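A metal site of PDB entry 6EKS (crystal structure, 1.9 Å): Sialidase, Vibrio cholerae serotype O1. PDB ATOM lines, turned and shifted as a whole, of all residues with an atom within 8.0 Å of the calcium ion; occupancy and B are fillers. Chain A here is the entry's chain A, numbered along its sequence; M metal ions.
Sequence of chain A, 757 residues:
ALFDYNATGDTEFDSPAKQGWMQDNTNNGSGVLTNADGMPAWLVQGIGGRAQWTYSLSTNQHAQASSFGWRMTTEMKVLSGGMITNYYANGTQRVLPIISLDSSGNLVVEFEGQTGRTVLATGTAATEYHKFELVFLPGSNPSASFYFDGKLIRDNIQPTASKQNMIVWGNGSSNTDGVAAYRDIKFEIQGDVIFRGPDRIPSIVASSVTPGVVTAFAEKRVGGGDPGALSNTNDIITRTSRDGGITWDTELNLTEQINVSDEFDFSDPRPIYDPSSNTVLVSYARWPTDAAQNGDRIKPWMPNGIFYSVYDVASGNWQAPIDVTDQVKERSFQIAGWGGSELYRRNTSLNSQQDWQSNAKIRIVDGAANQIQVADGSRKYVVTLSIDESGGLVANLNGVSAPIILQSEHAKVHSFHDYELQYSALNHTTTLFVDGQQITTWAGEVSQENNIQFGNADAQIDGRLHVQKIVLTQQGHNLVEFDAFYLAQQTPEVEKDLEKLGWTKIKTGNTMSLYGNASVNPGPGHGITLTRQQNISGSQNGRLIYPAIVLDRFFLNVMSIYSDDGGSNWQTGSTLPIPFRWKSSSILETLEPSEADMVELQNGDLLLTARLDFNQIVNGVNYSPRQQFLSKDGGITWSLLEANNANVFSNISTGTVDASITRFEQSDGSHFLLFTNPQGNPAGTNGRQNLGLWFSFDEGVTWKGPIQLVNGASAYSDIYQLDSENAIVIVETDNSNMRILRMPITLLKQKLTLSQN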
ATOM      1  N   VAL A 222      10.275   3.926 -19.928  1.00  0.00           N
ATOM      2  CA  VAL A 222      10.772   5.053 -19.155  1.00  0.00           C
ATOM      3  C   VAL A 222      10.662   4.647 -17.706  1.00  0.00           C
ATOM      4  O   VAL A 222       9.551   4.525 -17.165  1.00  0.00           O
ATOM      5  CB  VAL A 222       9.998   6.356 -19.417  1.00  0.00           C
ATOM      6  CG1 VAL A 222      10.474   7.459 -18.472  1.00  0.00           C
ATOM      7  CG2 VAL A 222      10.156   6.790 -20.892  1.00  0.00           C
ATOM      8  N   GLY A 224      12.233   1.743 -16.840  1.00  0.00           N
ATOM      9  CA  GLY A 224      12.624   0.347 -16.961  1.00  0.00           C
ATOM     10  C   GLY A 224      11.604  -0.672 -16.491  1.00  0.00           C
ATOM     11  O   GLY A 224      10.640  -0.327 -15.789  1.00  0.00           O
ATOM     12  N   GLY A 225      11.816  -1.926 -16.860  1.00  0.00           N
ATOM     13  CA  GLY A 225      11.015  -3.017 -16.316  1.00  0.00           C
ATOM     14  C   GLY A 225       9.699  -3.340 -17.041  1.00  0.00           C
ATOM     15  O   GLY A 225       9.266  -2.622 -17.944  1.00  0.00           O
ATOM     16  N   ASP A 226       9.064  -4.414 -16.596  1.00  0.00           N
ATOM     17  CA  ASP A 226       7.840  -4.920 -17.199  1.00  0.00           C
ATOM     18  C   ASP A 226       6.655  -3.972 -17.041  1.00  0.00           C
ATOM     19  O   ASP A 226       6.633  -3.142 -16.131  1.00  0.00           O
ATOM     20  CB  ASP A 226       7.497  -6.286 -16.614  1.00  0.00           C
ATOM     21  CG  ASP A 226       8.362  -7.391 -17.192  1.00  0.00           C
ATOM     22  OD1 ASP A 226       8.833  -7.231 -18.336  1.00  0.00           O
ATOM     23  OD2 ASP A 226       8.579  -8.399 -16.517  1.00  0.00           O
ATOM     24  N   PRO A 227       5.671  -4.095 -17.947  1.00  0.00           N
ATOM     25  CA  PRO A 227       4.467  -3.264 -17.769  1.00  0.00           C
ATOM     26  C   PRO A 227       3.771  -3.552 -16.425  1.00  0.00           C
ATOM     27  O   PRO A 227       3.904  -4.657 -15.868  1.00  0.00           O
ATOM     28  CB  PRO A 227       3.572  -3.672 -18.943  1.00  0.00           C
ATOM     29  CG  PRO A 227       4.053  -5.071 -19.341  1.00  0.00           C
ATOM     30  CD  PRO A 227       5.572  -4.986 -19.113  1.00  0.00           C
ATOM     31  N   GLY A 228       3.084  -2.552 -15.902  1.00  0.00           N
ATOM     32  CA  GLY A 228       2.299  -2.709 -14.685  1.00  0.00           C
ATOM     33  C   GLY A 228       2.948  -2.031 -13.489  1.00  0.00           C
ATOM     34  O   GLY A 228       2.379  -2.031 -12.407  1.00  0.00           O
ATOM     35  N   ALA A 229       4.154  -1.477 -13.653  1.00  0.00           N
ATOM     36  CA  ALA A 229       4.796  -0.834 -12.512  1.00  0.00           C
ATOM     37  C   ALA A 229       4.441   0.645 -12.482  1.00  0.00           C
ATOM     38  O   ALA A 229       4.489   1.308 -13.515  1.00  0.00           O
ATOM     39  CB  ALA A 229       6.344  -1.025 -12.543  1.00  0.00           C
ATOM     40  N   LEU A 230       4.143   1.144 -11.279  1.00  0.00           N
ATOM     41  CA  LEU A 230       3.872   2.564 -11.087  1.00  0.00           C
ATOM     42  C   LEU A 230       5.072   3.415 -11.504  1.00  0.00           C
ATOM     43  O   LEU A 230       4.939   4.549 -11.965  1.00  0.00           O
ATOM     44  CB  LEU A 230       3.503   2.839  -9.632  1.00  0.00           C
ATOM     45  CG  LEU A 230       2.724   4.112  -9.295  1.00  0.00           C
ATOM     46  CD1 LEU A 230       1.422   4.172 -10.089  1.00  0.00           C
ATOM     47  CD2 LEU A 230       2.436   4.201  -7.798  1.00  0.00           C
ATOM     48  N   SER A 231       6.266   2.843 -11.339  1.00  0.00           N
ATOM     49  CA  SER A 231       7.522   3.548 -11.572  1.00  0.00           C
ATOM     50  C   SER A 231       7.956   3.553 -13.034  1.00  0.00           C
ATOM     51  O   SER A 231       9.020   4.075 -13.369  1.00  0.00           O
ATOM     52  CB  SER A 231       8.640   2.955 -10.718  1.00  0.00           C
ATOM     53  OG  SER A 231       8.721   1.555 -10.947  1.00  0.00           O
ATOM     54  N   ASN A 232       7.154   2.964 -13.921  1.00  0.00           N
ATOM     55  CA  ASN A 232       7.481   3.164 -15.341  1.00  0.00           C
ATOM     56  C   ASN A 232       6.260   3.597 -16.178  1.00  0.00           C
ATOM     57  O   ASN A 232       5.127   3.456 -15.766  1.00  0.00           O
ATOM     58  CB  ASN A 232       8.148   1.907 -15.933  1.00  0.00           C
ATOM     59  CG  ASN A 232       7.255   0.671 -15.928  1.00  0.00           C
ATOM     60  OD1 ASN A 232       6.035   0.752 -15.970  1.00  0.00           O
ATOM     61  ND2 ASN A 232       7.883  -0.501 -15.929  1.00  0.00           N
ATOM     62  N   THR A 233       6.556   4.223 -17.310  1.00  0.00           N
ATOM     63  CA  THR A 233       5.569   4.493 -18.345  1.00  0.00           C
ATOM     64  C   THR A 233       6.112   3.904 -19.645  1.00  0.00           C
ATOM     65  O   THR A 233       7.126   4.382 -20.170  1.00  0.00           O
ATOM     66  CB  THR A 233       5.307   5.983 -18.541  1.00  0.00           C
ATOM     67  OG1 THR A 233       4.954   6.584 -17.285  1.00  0.00           O
ATOM     68  CG2 THR A 233       4.112   6.187 -19.535  1.00  0.00           C
ATOM     69  N   ASN A 234       5.480   2.839 -20.117  1.00  0.00           N
ATOM     70  CA  ASN A 234       5.998   2.103 -21.265  1.00  0.00           C
ATOM     71  C   ASN A 234       5.192   2.366 -22.531  1.00  0.00           C
ATOM     72  O   ASN A 234       3.961   2.388 -22.505  1.00  0.00           O
ATOM     73  CB  ASN A 234       6.024   0.597 -20.943  1.00  0.00           C
ATOM     74  CG  ASN A 234       6.994   0.254 -19.777  1.00  0.00           C
ATOM     75  OD1 ASN A 234       7.723   1.126 -19.301  1.00  0.00           O
ATOM     76  ND2 ASN A 234       7.006  -1.012 -19.354  1.00  0.00           N
ATOM     77  N   ASN A 259      -1.508   7.938 -24.830  1.00  0.00           N
ATOM     78  CA  ASN A 259      -0.996   7.784 -23.477  1.00  0.00           C
ATOM     79  C   ASN A 259      -0.732   9.179 -22.904  1.00  0.00           C
ATOM     80  O   ASN A 259       0.338   9.462 -22.367  1.00  0.00           O
ATOM     81  CB  ASN A 259       0.264   6.916 -23.503  1.00  0.00           C
ATOM     82  CG  ASN A 259       0.548   6.237 -22.157  1.00  0.00           C
ATOM     83  OD1 ASN A 259      -0.187   6.397 -21.190  1.00  0.00           O
ATOM     84  ND2 ASN A 259       1.626   5.463 -22.103  1.00  0.00           N
ATOM     85  N   ASP A 262       0.215   9.579 -19.270  1.00  0.00           N
ATOM     86  CA  ASP A 262       1.037   8.468 -18.813  1.00  0.00           C
ATOM     87  C   ASP A 262       0.208   7.521 -17.945  1.00  0.00           C
ATOM     88  O   ASP A 262       0.707   6.987 -16.963  1.00  0.00           O
ATOM     89  CB  ASP A 262       2.259   8.964 -18.037  1.00  0.00           C
ATOM     90  CG  ASP A 262       3.192   9.799 -18.883  1.00  0.00           C
ATOM     91  OD1 ASP A 262       3.179   9.656 -20.120  1.00  0.00           O
ATOM     92  OD2 ASP A 262       3.972  10.580 -18.318  1.00  0.00           O
ATOM     93  N   GLU A 263      -1.048   7.298 -18.309  1.00  0.00           N
ATOM     94  CA  GLU A 263      -1.917   6.458 -17.483  1.00  0.00           C
ATOM     95  C   GLU A 263      -1.794   4.989 -17.886  1.00  0.00           C
ATOM     96  O   GLU A 263      -2.324   4.113 -17.210  1.00  0.00           O
ATOM     97  CB  GLU A 263      -3.373   6.939 -17.588  1.00  0.00           C
ATOM     98  CG  GLU A 263      -3.960   6.749 -18.970  1.00  0.00           C
ATOM     99  CD  GLU A 263      -3.865   7.983 -19.904  1.00  0.00           C
ATOM    100  OE1 GLU A 263      -4.919   8.345 -20.490  1.00  0.00           O
ATOM    101  OE2 GLU A 263      -2.761   8.568 -20.075  1.00  0.00           O
ATOM    102  N   PHE A 264      -1.056   4.723 -18.972  1.00  0.00           N
ATOM    103  CA  PHE A 264      -0.967   3.355 -19.512  1.00  0.00           C
ATOM    104  C   PHE A 264       0.450   2.892 -19.701  1.00  0.00           C
ATOM    105  O   PHE A 264       1.361   3.707 -19.809  1.00  0.00           O
ATOM    106  CB  PHE A 264      -1.645   3.249 -20.894  1.00  0.00           C
ATOM    107  CG  PHE A 264      -3.067   3.642 -20.895  1.00  0.00           C
ATOM    108  CD1 PHE A 264      -4.008   2.938 -20.145  1.00  0.00           C
ATOM    109  CD2 PHE A 264      -3.498   4.689 -21.697  1.00  0.00           C
ATOM    110  CE1 PHE A 264      -5.344   3.297 -20.167  1.00  0.00           C
ATOM    111  CE2 PHE A 264      -4.827   5.036 -21.714  1.00  0.00           C
ATOM    112  CZ  PHE A 264      -5.748   4.355 -20.959  1.00  0.00           C
ATOM    113  N   ASP A 265       0.617   1.574 -19.741  1.00  0.00           N
ATOM    114  CA  ASP A 265       1.801   0.942 -20.315  1.00  0.00           C
ATOM    115  C   ASP A 265       1.373   0.190 -21.574  1.00  0.00           C
ATOM    116  O   ASP A 265       0.323  -0.453 -21.572  1.00  0.00           O
ATOM    117  CB  ASP A 265       2.464  -0.053 -19.362  1.00  0.00           C
ATOM    118  CG  ASP A 265       3.040   0.598 -18.122  1.00  0.00           C
ATOM    119  OD1 ASP A 265       3.676   1.679 -18.239  1.00  0.00           O
ATOM    120  OD2 ASP A 265       2.874  -0.007 -17.027  1.00  0.00           O
ATOM    121  N   PHE A 266       2.192   0.210 -22.615  1.00  0.00           N
ATOM    122  CA  PHE A 266       1.942  -0.644 -23.765  1.00  0.00           C
ATOM    123  C   PHE A 266       3.069  -1.651 -23.873  1.00  0.00           C
ATOM    124  O   PHE A 266       4.198  -1.374 -23.442  1.00  0.00           O
ATOM    125  CB  PHE A 266       1.786   0.200 -25.043  1.00  0.00           C
ATOM    126  CG  PHE A 266       0.618   1.149 -24.997  1.00  0.00           C
ATOM    127  CD1 PHE A 266       0.736   2.388 -24.377  1.00  0.00           C
ATOM    128  CD2 PHE A 266      -0.614   0.791 -25.566  1.00  0.00           C
ATOM    129  CE1 PHE A 266      -0.346   3.265 -24.336  1.00  0.00           C
ATOM    130  CE2 PHE A 266      -1.694   1.673 -25.538  1.00  0.00           C
ATOM    131  CZ  PHE A 266      -1.569   2.900 -24.913  1.00  0.00           C
ATOM    132  N   TRP A 287      -2.059  -1.752 -21.068  1.00  0.00           N
ATOM    133  CA  TRP A 287      -2.274  -2.037 -19.637  1.00  0.00           C
ATOM    134  C   TRP A 287      -2.479  -0.733 -18.882  1.00  0.00           C
ATOM    135  O   TRP A 287      -1.877   0.278 -19.258  1.00  0.00           O
ATOM    136  CB  TRP A 287      -1.067  -2.765 -19.022  1.00  0.00           C
ATOM    137  CG  TRP A 287      -0.534  -3.908 -19.826  1.00  0.00           C
ATOM    138  CD1 TRP A 287       0.444  -3.859 -20.770  1.00  0.00           C
ATOM    139  CD2 TRP A 287      -0.940  -5.273 -19.725  1.00  0.00           C
ATOM    140  NE1 TRP A 287       0.652  -5.112 -21.287  1.00  0.00           N
ATOM    141  CE2 TRP A 287      -0.186  -6.002 -20.661  1.00  0.00           C
ATOM    142  CE3 TRP A 287      -1.906  -5.953 -18.962  1.00  0.00           C
ATOM    143  CZ2 TRP A 287      -0.335  -7.380 -20.832  1.00  0.00           C
ATOM    144  CZ3 TRP A 287      -2.038  -7.323 -19.119  1.00  0.00           C
ATOM    145  CH2 TRP A 287      -1.285  -8.019 -20.057  1.00  0.00           C
ATOM    146  N   PRO A 288      -3.259  -0.744 -17.792  1.00  0.00           N
ATOM    147  CA  PRO A 288      -3.121   0.409 -16.908  1.00  0.00           C
ATOM    148  C   PRO A 288      -1.663   0.454 -16.421  1.00  0.00           C
ATOM    149  O   PRO A 288      -1.051  -0.600 -16.253  1.00  0.00           O
ATOM    150  CB  PRO A 288      -4.085   0.101 -15.755  1.00  0.00           C
ATOM    151  CG  PRO A 288      -4.142  -1.394 -15.723  1.00  0.00           C
ATOM    152  CD  PRO A 288      -3.972  -1.863 -17.141  1.00  0.00           C
ATOM    153  N   THR A 289      -1.113   1.646 -16.208  1.00  0.00           N
ATOM    154  CA  THR A 289       0.317   1.748 -15.913  1.00  0.00           C
ATOM    155  C   THR A 289       0.678   1.055 -14.588  1.00  0.00           C
ATOM    156  O   THR A 289       1.850   0.723 -14.355  1.00  0.00           O
ATOM    157  CB  THR A 289       0.772   3.220 -15.907  1.00  0.00           C
ATOM    158  OG1 THR A 289       2.187   3.295 -15.835  1.00  0.00           O
ATOM    159  CG2 THR A 289       0.163   3.981 -14.714  1.00  0.00           C
ATOM    160  N   ASP A 290      -0.314   0.832 -13.732  1.00  0.00           N
ATOM    161  CA  ASP A 290      -0.020   0.257 -12.427  1.00  0.00           C
ATOM    162  C   ASP A 290      -0.475  -1.201 -12.241  1.00  0.00           C
ATOM    163  O   ASP A 290      -0.421  -1.722 -11.116  1.00  0.00           O
ATOM    164  CB  ASP A 290      -0.611   1.136 -11.314  1.00  0.00           C
ATOM    165  CG  ASP A 290      -2.123   1.291 -11.406  1.00  0.00           C
ATOM    166  OD1 ASP A 290      -2.710   0.892 -12.431  1.00  0.00           O
ATOM    167  OD2 ASP A 290      -2.726   1.817 -10.445  1.00  0.00           O
ATOM    168  N   ALA A 291      -0.840  -1.900 -13.304  1.00  0.00           N
ATOM    169  CA  ALA A 291      -1.140  -3.316 -13.141  1.00  0.00           C
ATOM    170  C   ALA A 291      -1.107  -4.047 -14.458  1.00  0.00           C
ATOM    171  O   ALA A 291      -1.707  -3.597 -15.454  1.00  0.00           O
ATOM    172  CB  ALA A 291      -2.530  -3.518 -12.462  1.00  0.00           C
ATOM    173  N   ALA A 292      -0.475  -5.208 -14.484  1.00  0.00           N
ATOM    174  CA  ALA A 292      -0.427  -5.963 -15.730  1.00  0.00           C
ATOM    175  C   ALA A 292      -0.341  -7.464 -15.487  1.00  0.00           C
ATOM    176  O   ALA A 292      -0.883  -7.989 -14.517  1.00  0.00           O
ATOM    177  CB  ALA A 292       0.766  -5.474 -16.618  1.00  0.00           C
ATOM    178  N   ARG A 297      -1.952  -9.450 -11.673  1.00  0.00           N
ATOM    179  CA  ARG A 297      -2.567  -8.317 -10.989  1.00  0.00           C
ATOM    180  C   ARG A 297      -3.676  -7.662 -11.831  1.00  0.00           C
ATOM    181  O   ARG A 297      -4.585  -7.057 -11.285  1.00  0.00           O
ATOM    182  CB  ARG A 297      -1.502  -7.292 -10.595  1.00  0.00           C
ATOM    183  CG  ARG A 297      -0.570  -7.853  -9.463  1.00  0.00           C
ATOM    184  CD  ARG A 297       0.047  -6.715  -8.647  1.00  0.00           C
ATOM    185  NE  ARG A 297       0.990  -5.935  -9.428  1.00  0.00           N
ATOM    186  CZ  ARG A 297       0.746  -4.716  -9.900  1.00  0.00           C
ATOM    187  NH1 ARG A 297      -0.425  -4.138  -9.640  1.00  0.00           N
ATOM    188  NH2 ARG A 297       1.675  -4.083 -10.611  1.00  0.00           N
HETATM  189 CA    CA M   1       3.789   1.560 -15.663  1.00  0.00          CA
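Within 4 Å of the calcium ion: Ala 229, Asn 232, Asp 265 and Thr 289.
Along chain A the residues within 4 Å of the calcium ion span positions 229 to 289.
The nearest printed residue that does not touch the calcium ion is Thr 233 (4.2 Å).
The calcium ion is bound by the side-chain carboxylate (OD2) of Asp 265, the backbone carbonyl oxygen (O) of Ala 229, the backbone carbonyl oxygen (O) of Asn 232, the side-chain hydroxyl (OG1) of Thr 289, the side-chain amide oxygen (OD1) of Asn 232, the backbone carbonyl oxygen (O) of Thr 289 and the side-chain carboxylate (OD1) of Asp 265.
The calcium ion has seven donor atoms within binding distance.
N of Gly 228 lies close to OD2 of Asp 265 (2.8 Å).
OD1 of Asp 265 sits close to N of Asn 234 (2.9 Å).
O of Asp 265 is in hydrogen-bond range of N of Trp 287 (2.8 Å).
The side-chain amide nitrogen of Asn 232 sits at hydrogen-bond distance from the backbone carbonyl oxygen of Asp 226 (2.9 Å).
ND2 of Asn 232 sits at hydrogen-bond distance from O of Gly 224 (2.8 Å).
The side-chain amide nitrogen (ND2) of Asn 232 is in hydrogen-bond range of the backbone carbonyl oxygen (O) of Gly 225 (3.2 Å).
N of Thr 289 lies within hydrogen-bond range of O of Glu 263 (2.9 Å).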
